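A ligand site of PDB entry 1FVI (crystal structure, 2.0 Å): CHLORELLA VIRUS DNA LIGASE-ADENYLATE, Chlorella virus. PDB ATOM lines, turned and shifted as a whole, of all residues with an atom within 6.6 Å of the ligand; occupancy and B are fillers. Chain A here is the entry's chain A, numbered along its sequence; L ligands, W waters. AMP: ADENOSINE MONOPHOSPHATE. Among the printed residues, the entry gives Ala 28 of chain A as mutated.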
ATOM      1  N   LEU A   6      33.727 -25.220  16.963  1.00  0.00           N
ATOM      2  CA  LEU A   6      33.782 -26.650  17.225  1.00  0.00           C
ATOM      3  C   LEU A   6      32.833 -27.315  16.209  1.00  0.00           C
ATOM      4  O   LEU A   6      31.665 -26.919  16.083  1.00  0.00           O
ATOM      5  CB  LEU A   6      33.275 -26.919  18.648  1.00  0.00           C
ATOM      6  CG  LEU A   6      33.551 -28.215  19.426  1.00  0.00           C
ATOM      7  CD1 LEU A   6      32.432 -28.390  20.445  1.00  0.00           C
ATOM      8  CD2 LEU A   6      33.657 -29.448  18.544  1.00  0.00           C
ATOM      9  N   LEU A   7      33.342 -28.285  15.467  1.00  0.00           N
ATOM     10  CA  LEU A   7      32.519 -29.001  14.501  1.00  0.00           C
ATOM     11  C   LEU A   7      32.340 -30.472  14.916  1.00  0.00           C
ATOM     12  O   LEU A   7      33.050 -30.987  15.778  1.00  0.00           O
ATOM     13  CB  LEU A   7      33.096 -28.851  13.095  1.00  0.00           C
ATOM     14  CG  LEU A   7      33.187 -27.387  12.668  1.00  0.00           C
ATOM     15  CD1 LEU A   7      33.869 -27.296  11.319  1.00  0.00           C
ATOM     16  CD2 LEU A   7      31.788 -26.742  12.639  1.00  0.00           C
ATOM     17  N   ALA A   8      31.335 -31.104  14.332  1.00  0.00           N
ATOM     18  CA  ALA A   8      31.010 -32.480  14.664  1.00  0.00           C
ATOM     19  C   ALA A   8      31.402 -33.564  13.680  1.00  0.00           C
ATOM     20  O   ALA A   8      31.515 -33.340  12.470  1.00  0.00           O
ATOM     21  CB  ALA A   8      29.475 -32.592  14.946  1.00  0.00           C
ATOM     22  N   THR A  10      30.358 -37.392  12.261  1.00  0.00           N
ATOM     23  CA  THR A  10      29.066 -38.040  12.045  1.00  0.00           C
ATOM     24  C   THR A  10      28.989 -39.409  12.731  1.00  0.00           C
ATOM     25  O   THR A  10      29.938 -40.207  12.676  1.00  0.00           O
ATOM     26  CB  THR A  10      28.773 -38.186  10.553  1.00  0.00           C
ATOM     27  OG1 THR A  10      28.720 -36.888   9.970  1.00  0.00           O
ATOM     28  CG2 THR A  10      27.436 -38.922  10.307  1.00  0.00           C
ATOM     29  N   THR A  24      21.628 -32.604  22.669  1.00  0.00           N
ATOM     30  CA  THR A  24      20.874 -31.383  22.381  1.00  0.00           C
ATOM     31  C   THR A  24      20.296 -31.575  20.975  1.00  0.00           C
ATOM     32  O   THR A  24      20.661 -32.529  20.279  1.00  0.00           O
ATOM     33  CB  THR A  24      21.761 -30.095  22.446  1.00  0.00           C
ATOM     34  OG1 THR A  24      22.930 -30.247  21.632  1.00  0.00           O
ATOM     35  CG2 THR A  24      22.140 -29.738  23.895  1.00  0.00           C
ATOM     36  N   PRO A  25      19.338 -30.720  20.590  1.00  0.00           N
ATOM     37  CA  PRO A  25      18.729 -30.836  19.256  1.00  0.00           C
ATOM     38  C   PRO A  25      19.569 -30.266  18.140  1.00  0.00           C
ATOM     39  O   PRO A  25      20.218 -29.224  18.301  1.00  0.00           O
ATOM     40  CB  PRO A  25      17.425 -30.078  19.414  1.00  0.00           C
ATOM     41  CG  PRO A  25      17.784 -28.999  20.362  1.00  0.00           C
ATOM     42  CD  PRO A  25      18.600 -29.742  21.399  1.00  0.00           C
ATOM     43  N   LYS A  26      19.595 -30.973  17.018  1.00  0.00           N
ATOM     44  CA  LYS A  26      20.333 -30.505  15.843  1.00  0.00           C
ATOM     45  C   LYS A  26      19.503 -29.365  15.228  1.00  0.00           C
ATOM     46  O   LYS A  26      18.410 -29.582  14.684  1.00  0.00           O
ATOM     47  CB  LYS A  26      20.541 -31.659  14.852  1.00  0.00           C
ATOM     48  CG  LYS A  26      21.537 -31.405  13.709  1.00  0.00           C
ATOM     49  CD  LYS A  26      21.696 -32.679  12.905  1.00  0.00           C
ATOM     50  CE  LYS A  26      22.851 -32.640  11.884  1.00  0.00           C
ATOM     51  NZ  LYS A  26      22.700 -31.620  10.798  1.00  0.00           N
ATOM     52  N   ILE A  27      19.999 -28.141  15.362  1.00  0.00           N
ATOM     53  CA  ILE A  27      19.327 -26.961  14.828  1.00  0.00           C
ATOM     54  C   ILE A  27      19.747 -26.605  13.395  1.00  0.00           C
ATOM     55  O   ILE A  27      20.950 -26.626  13.036  1.00  0.00           O
ATOM     56  CB  ILE A  27      19.558 -25.726  15.757  1.00  0.00           C
ATOM     57  CG1 ILE A  27      19.065 -26.033  17.171  1.00  0.00           C
ATOM     58  CG2 ILE A  27      18.868 -24.474  15.215  1.00  0.00           C
ATOM     59  CD1 ILE A  27      19.822 -25.288  18.221  1.00  0.00           C
ATOM     60  N   ALA A  28      18.742 -26.300  12.583  1.00  0.00           N
ATOM     61  CA  ALA A  28      18.933 -25.873  11.203  1.00  0.00           C
ATOM     62  C   ALA A  28      18.965 -24.353  11.342  1.00  0.00           C
ATOM     63  O   ALA A  28      17.928 -23.710  11.536  1.00  0.00           O
ATOM     64  CB  ALA A  28      17.755 -26.316  10.338  1.00  0.00           C
ATOM     65  N   GLY A  29      20.156 -23.776  11.335  1.00  0.00           N
ATOM     66  CA  GLY A  29      20.234 -22.332  11.479  1.00  0.00           C
ATOM     67  C   GLY A  29      21.579 -21.761  11.107  1.00  0.00           C
ATOM     68  O   GLY A  29      22.366 -22.389  10.381  1.00  0.00           O
ATOM     69  N   ARG A  31      25.062 -20.688  12.460  1.00  0.00           N
ATOM     70  CA  ARG A  31      26.063 -20.831  13.532  1.00  0.00           C
ATOM     71  C   ARG A  31      26.652 -19.435  13.815  1.00  0.00           C
ATOM     72  O   ARG A  31      27.082 -18.717  12.885  1.00  0.00           O
ATOM     73  CB  ARG A  31      27.185 -21.775  13.097  1.00  0.00           C
ATOM     74  CG  ARG A  31      28.233 -22.063  14.151  1.00  0.00           C
ATOM     75  CD  ARG A  31      27.589 -22.770  15.349  1.00  0.00           C
ATOM     76  NE  ARG A  31      28.566 -23.193  16.349  1.00  0.00           N
ATOM     77  CZ  ARG A  31      29.320 -24.283  16.255  1.00  0.00           C
ATOM     78  NH1 ARG A  31      29.211 -25.068  15.188  1.00  0.00           N
ATOM     79  NH2 ARG A  31      30.189 -24.591  17.215  1.00  0.00           N
ATOM     80  N   ARG A  41      30.277 -18.918  11.036  1.00  0.00           N
ATOM     81  CA  ARG A  41      31.206 -20.044  11.087  1.00  0.00           C
ATOM     82  C   ARG A  41      32.547 -19.763  10.426  1.00  0.00           C
ATOM     83  O   ARG A  41      33.557 -20.362  10.791  1.00  0.00           O
ATOM     84  CB  ARG A  41      30.604 -21.327  10.513  1.00  0.00           C
ATOM     85  CG  ARG A  41      30.300 -21.331   9.047  1.00  0.00           C
ATOM     86  CD  ARG A  41      29.667 -22.667   8.661  1.00  0.00           C
ATOM     87  NE  ARG A  41      30.655 -23.744   8.521  1.00  0.00           N
ATOM     88  CZ  ARG A  41      30.477 -24.989   8.948  1.00  0.00           C
ATOM     89  NH1 ARG A  41      29.353 -25.325   9.563  1.00  0.00           N
ATOM     90  NH2 ARG A  41      31.382 -25.911   8.676  1.00  0.00           N
ATOM     91  N   GLU A  66      23.193 -20.931  17.756  1.00  0.00           N
ATOM     92  CA  GLU A  66      22.536 -20.870  16.455  1.00  0.00           C
ATOM     93  C   GLU A  66      21.441 -19.815  16.375  1.00  0.00           C
ATOM     94  O   GLU A  66      20.535 -19.752  17.226  1.00  0.00           O
ATOM     95  CB  GLU A  66      21.877 -22.232  16.134  1.00  0.00           C
ATOM     96  CG  GLU A  66      22.824 -23.419  15.908  1.00  0.00           C
ATOM     97  CD  GLU A  66      23.309 -23.524  14.491  1.00  0.00           C
ATOM     98  OE1 GLU A  66      24.316 -24.204  14.268  1.00  0.00           O
ATOM     99  OE2 GLU A  66      22.677 -22.971  13.567  1.00  0.00           O
ATOM    100  N   PHE A  97      24.135 -22.715  22.928  1.00  0.00           N
ATOM    101  CA  PHE A  97      24.538 -24.035  23.389  1.00  0.00           C
ATOM    102  C   PHE A  97      25.928 -24.198  24.026  1.00  0.00           C
ATOM    103  O   PHE A  97      26.222 -25.264  24.571  1.00  0.00           O
ATOM    104  CB  PHE A  97      24.303 -25.091  22.292  1.00  0.00           C
ATOM    105  CG  PHE A  97      24.965 -24.785  20.973  1.00  0.00           C
ATOM    106  CD1 PHE A  97      26.368 -24.715  20.864  1.00  0.00           C
ATOM    107  CD2 PHE A  97      24.193 -24.683  19.818  1.00  0.00           C
ATOM    108  CE1 PHE A  97      26.992 -24.561  19.627  1.00  0.00           C
ATOM    109  CE2 PHE A  97      24.801 -24.535  18.567  1.00  0.00           C
ATOM    110  CZ  PHE A  97      26.196 -24.470  18.456  1.00  0.00           C
ATOM    111  N   LEU A 136      20.386 -23.834  25.501  1.00  0.00           N
ATOM    112  CA  LEU A 136      20.319 -25.229  25.124  1.00  0.00           C
ATOM    113  C   LEU A 136      21.064 -26.047  26.148  1.00  0.00           C
ATOM    114  O   LEU A 136      22.255 -26.302  26.008  1.00  0.00           O
ATOM    115  CB  LEU A 136      20.941 -25.458  23.753  1.00  0.00           C
ATOM    116  CG  LEU A 136      20.096 -25.514  22.478  1.00  0.00           C
ATOM    117  CD1 LEU A 136      20.852 -26.369  21.461  1.00  0.00           C
ATOM    118  CD2 LEU A 136      18.710 -26.123  22.731  1.00  0.00           C
ATOM    119  N   GLU A 160      16.356 -31.126  13.255  1.00  0.00           N
ATOM    120  CA  GLU A 160      16.969 -32.039  12.271  1.00  0.00           C
ATOM    121  C   GLU A 160      17.358 -33.424  12.756  1.00  0.00           C
ATOM    122  O   GLU A 160      17.391 -34.379  11.991  1.00  0.00           O
ATOM    123  CB  GLU A 160      18.251 -31.402  11.677  1.00  0.00           C
ATOM    124  CG  GLU A 160      18.075 -30.108  10.894  1.00  0.00           C
ATOM    125  CD  GLU A 160      17.219 -30.303   9.662  1.00  0.00           C
ATOM    126  OE1 GLU A 160      16.009 -29.973   9.706  1.00  0.00           O
ATOM    127  OE2 GLU A 160      17.753 -30.780   8.639  1.00  0.00           O
ATOM    128  N   MET A 163      22.448 -33.804  18.499  1.00  0.00           N
ATOM    129  CA  MET A 163      23.874 -33.512  18.679  1.00  0.00           C
ATOM    130  C   MET A 163      24.308 -34.140  20.006  1.00  0.00           C
ATOM    131  O   MET A 163      23.704 -33.887  21.043  1.00  0.00           O
ATOM    132  CB  MET A 163      24.128 -31.997  18.684  1.00  0.00           C
ATOM    133  CG  MET A 163      23.674 -31.299  17.403  1.00  0.00           C
ATOM    134  SD  MET A 163      24.451 -31.910  15.893  1.00  0.00           S
ATOM    135  CE  MET A 163      26.167 -31.365  16.122  1.00  0.00           C
ATOM    136  N   ARG A 165      27.412 -35.068  22.892  1.00  0.00           N
ATOM    137  CA  ARG A 165      28.657 -34.614  23.492  1.00  0.00           C
ATOM    138  C   ARG A 165      29.053 -35.381  24.741  1.00  0.00           C
ATOM    139  O   ARG A 165      28.197 -35.723  25.580  1.00  0.00           O
ATOM    140  CB  ARG A 165      28.566 -33.129  23.885  1.00  0.00           C
ATOM    141  CG  ARG A 165      28.287 -32.157  22.756  1.00  0.00           C
ATOM    142  CD  ARG A 165      29.066 -30.881  22.974  1.00  0.00           C
ATOM    143  NE  ARG A 165      28.400 -29.705  22.427  1.00  0.00           N
ATOM    144  CZ  ARG A 165      28.937 -28.477  22.405  1.00  0.00           C
ATOM    145  NH1 ARG A 165      30.160 -28.261  22.878  1.00  0.00           N
ATOM    146  NH2 ARG A 165      28.219 -27.449  21.988  1.00  0.00           N
ATOM    147  N   ARG A 175      37.085 -29.726  13.903  1.00  0.00           N
ATOM    148  CA  ARG A 175      36.089 -30.787  13.898  1.00  0.00           C
ATOM    149  C   ARG A 175      36.481 -31.997  14.761  1.00  0.00           C
ATOM    150  O   ARG A 175      37.578 -32.513  14.673  1.00  0.00           O
ATOM    151  CB  ARG A 175      35.801 -31.224  12.474  1.00  0.00           C
ATOM    152  CG  ARG A 175      34.643 -32.215  12.330  1.00  0.00           C
ATOM    153  CD  ARG A 175      34.447 -32.584  10.858  1.00  0.00           C
ATOM    154  NE  ARG A 175      33.480 -31.742  10.143  1.00  0.00           N
ATOM    155  CZ  ARG A 175      33.736 -30.541   9.626  1.00  0.00           C
ATOM    156  NH1 ARG A 175      34.953 -30.014   9.727  1.00  0.00           N
ATOM    157  NH2 ARG A 175      32.750 -29.868   9.051  1.00  0.00           N
ATOM    158  N   LEU A 183      31.904 -33.895  19.921  1.00  0.00           N
ATOM    159  CA  LEU A 183      30.688 -33.379  19.309  1.00  0.00           C
ATOM    160  C   LEU A 183      30.360 -34.297  18.149  1.00  0.00           C
ATOM    161  O   LEU A 183      31.169 -34.432  17.242  1.00  0.00           O
ATOM    162  CB  LEU A 183      30.882 -31.931  18.803  1.00  0.00           C
ATOM    163  CG  LEU A 183      29.709 -30.951  18.778  1.00  0.00           C
ATOM    164  CD1 LEU A 183      29.628 -30.338  17.398  1.00  0.00           C
ATOM    165  CD2 LEU A 183      28.353 -31.573  19.258  1.00  0.00           C
ATOM    166  N   LYS A 185      27.092 -35.685  15.383  1.00  0.00           N
ATOM    167  CA  LYS A 185      25.764 -35.467  14.839  1.00  0.00           C
ATOM    168  C   LYS A 185      25.119 -36.797  14.478  1.00  0.00           C
ATOM    169  O   LYS A 185      25.752 -37.700  13.922  1.00  0.00           O
ATOM    170  CB  LYS A 185      25.755 -34.450  13.680  1.00  0.00           C
ATOM    171  CG  LYS A 185      26.781 -34.603  12.601  1.00  0.00           C
ATOM    172  CD  LYS A 185      26.767 -33.354  11.725  1.00  0.00           C
ATOM    173  CE  LYS A 185      27.507 -33.570  10.423  1.00  0.00           C
ATOM    174  NZ  LYS A 185      27.328 -32.419   9.491  1.00  0.00           N
ATOM    175  N   LYS A 187      21.550 -38.685  12.913  1.00  0.00           N
ATOM    176  CA  LYS A 187      20.297 -38.677  12.174  1.00  0.00           C
ATOM    177  C   LYS A 187      20.074 -40.167  11.877  1.00  0.00           C
ATOM    178  O   LYS A 187      20.441 -40.674  10.822  1.00  0.00           O
ATOM    179  CB  LYS A 187      20.412 -37.812  10.913  1.00  0.00           C
ATOM    180  CG  LYS A 187      20.530 -36.311  11.218  1.00  0.00           C
ATOM    181  CD  LYS A 187      20.983 -35.494  10.024  1.00  0.00           C
ATOM    182  CE  LYS A 187      19.937 -35.444   8.930  1.00  0.00           C
ATOM    183  NZ  LYS A 187      20.411 -34.682   7.742  1.00  0.00           N
HETATM  184  P   AMP L   1      23.819 -31.127   9.981  1.00  0.00           P
HETATM  185  O1P AMP L   1      24.616 -32.095   9.243  1.00  0.00           O
HETATM  186  O3P AMP L   1      23.502 -30.097   8.815  1.00  0.00           O
HETATM  187  O5' AMP L   1      24.702 -30.306  10.886  1.00  0.00           O
HETATM  188  C5' AMP L   1      24.128 -29.118  11.637  1.00  0.00           C
HETATM  189  C4' AMP L   1      25.147 -28.034  11.898  1.00  0.00           C
HETATM  190  O4' AMP L   1      24.595 -27.222  12.931  1.00  0.00           O
HETATM  191  C3' AMP L   1      26.501 -28.577  12.425  1.00  0.00           C
HETATM  192  O3' AMP L   1      27.645 -27.875  11.924  1.00  0.00           O
HETATM  193  C2' AMP L   1      26.453 -28.341  13.895  1.00  0.00           C
HETATM  194  O2' AMP L   1      27.750 -28.082  14.397  1.00  0.00           O
HETATM  195  C1' AMP L   1      25.436 -27.195  14.070  1.00  0.00           C
HETATM  196  N9  AMP L   1      24.606 -27.419  15.245  1.00  0.00           N
HETATM  197  C8  AMP L   1      23.234 -27.357  15.250  1.00  0.00           C
HETATM  198  N7  AMP L   1      22.772 -27.594  16.442  1.00  0.00           N
HETATM  199  C5  AMP L   1      23.856 -27.823  17.278  1.00  0.00           C
HETATM  200  C6  AMP L   1      23.978 -28.124  18.644  1.00  0.00           C
HETATM  201  N6  AMP L   1      22.914 -28.259  19.458  1.00  0.00           N
HETATM  202  N1  AMP L   1      25.228 -28.279  19.110  1.00  0.00           N
HETATM  203  C2  AMP L   1      26.263 -28.145  18.308  1.00  0.00           C
HETATM  204  N3  AMP L   1      26.295 -27.862  16.995  1.00  0.00           N
HETATM  205  C4  AMP L   1      25.036 -27.699  16.500  1.00  0.00           C
HETATM  206  O   HOH W   1      22.409 -25.748  11.138  1.00  0.00           O
HETATM  207  O   HOH W   2      27.772 -24.888  12.608  1.00  0.00           O
HETATM  208  O   HOH W   3      24.565 -24.149  11.642  1.00  0.00           O
HETATM  209  O   HOH W   4      29.355 -29.883  12.753  1.00  0.00           O
HETATM  210  O   HOH W   5      25.408 -28.645   7.680  1.00  0.00           O
HETATM  211  O   HOH W   6      25.841 -28.923  21.653  1.00  0.00           O
HETATM  212  O   HOH W   7      21.892 -28.142   8.917  1.00  0.00           O
HETATM  213  O   HOH W   8      23.855 -34.748   9.391  1.00  0.00           O
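OG1 of Thr 24 is in hydrogen-bond range of N6 of the ligand (2.9 Å).
The backbone NH (N) of Ile 27 is in hydrogen-bond range of a nitrogen (N7) of the ligand (3.0 Å).
The backbone carbonyl oxygen (O) of Pro 25 sits at hydrogen-bond distance from a nitrogen (N6) of the ligand (3.1 Å).
O2' of the ligand sits at hydrogen-bond distance from NH1 of Arg 31 (3.4 Å).
The side-chain amino group (NZ) of Lys 185 lies within salt-bridge range of an oxygen (O1P) of the ligand (2.7 Å).
The side-chain amino group of Lys 26 is covalently linked to a phosphorus (P) of the ligand, 1.5 Å away.
The guanidinium group (NH2) of Arg 31 is in hydrogen-bond range of the backbone carbonyl oxygen (O) of Leu 6 (3.0 Å).
The side-chain carboxylate of Glu 66 lies within hydrogen-bond range of the backbone NH of Arg 31, 3.5 Å away.
The backbone NH of Glu 160 is in hydrogen-bond range of the backbone carbonyl oxygen of Lys 26.
The backbone carbonyl oxygen (O) of Thr 24 is in hydrogen-bond range of the backbone NH (N) of Met 163, at 2.8 Å.
OE2 of Glu 66 lies close to N of Gly 29, 3.5 Å away.
Water W6 lies within hydrogen-bond range of a nitrogen (N1) of the ligand (2.7 Å), the guanidinium group of Arg 165 (2.8 Å) and the side-chain hydroxyl of Thr 24 (3.2 Å).
Water W4 bridges O3' of the ligand (2.8 Å) and N of Ala 8 (2.8 Å).
Water W2 lies within hydrogen-bond range of the guanidinium group of Arg 31, an oxygen (O3') of the ligand and the guanidinium group of Arg 41.
Water W1 lies within hydrogen-bond range of the backbone carbonyl oxygen of Ile 27 (2.5 Å), the backbone NH of Gly 29 (3.0 Å) and an oxygen (O4') of the ligand (3.2 Å).
An oxygen (O4') of the ligand sits close to the side-chain carboxylate (OE1) of Glu 66 (3.3 Å).
Residues that only touch the ligand: Arg 41, Phe 97, Leu 136 and Met 163.
Hydrophobic or aromatic side chains that line the ligand: Ile 27, Phe 97, Leu 136 and Met 163.
Of the 22 residues printed, 11 come within 4 Å of the ligand.
Along chain A the residues within 4 Å of the ligand span positions 24 to 185.
The nearest printed residue that does not touch the ligand is Leu 183 (4.1 Å).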
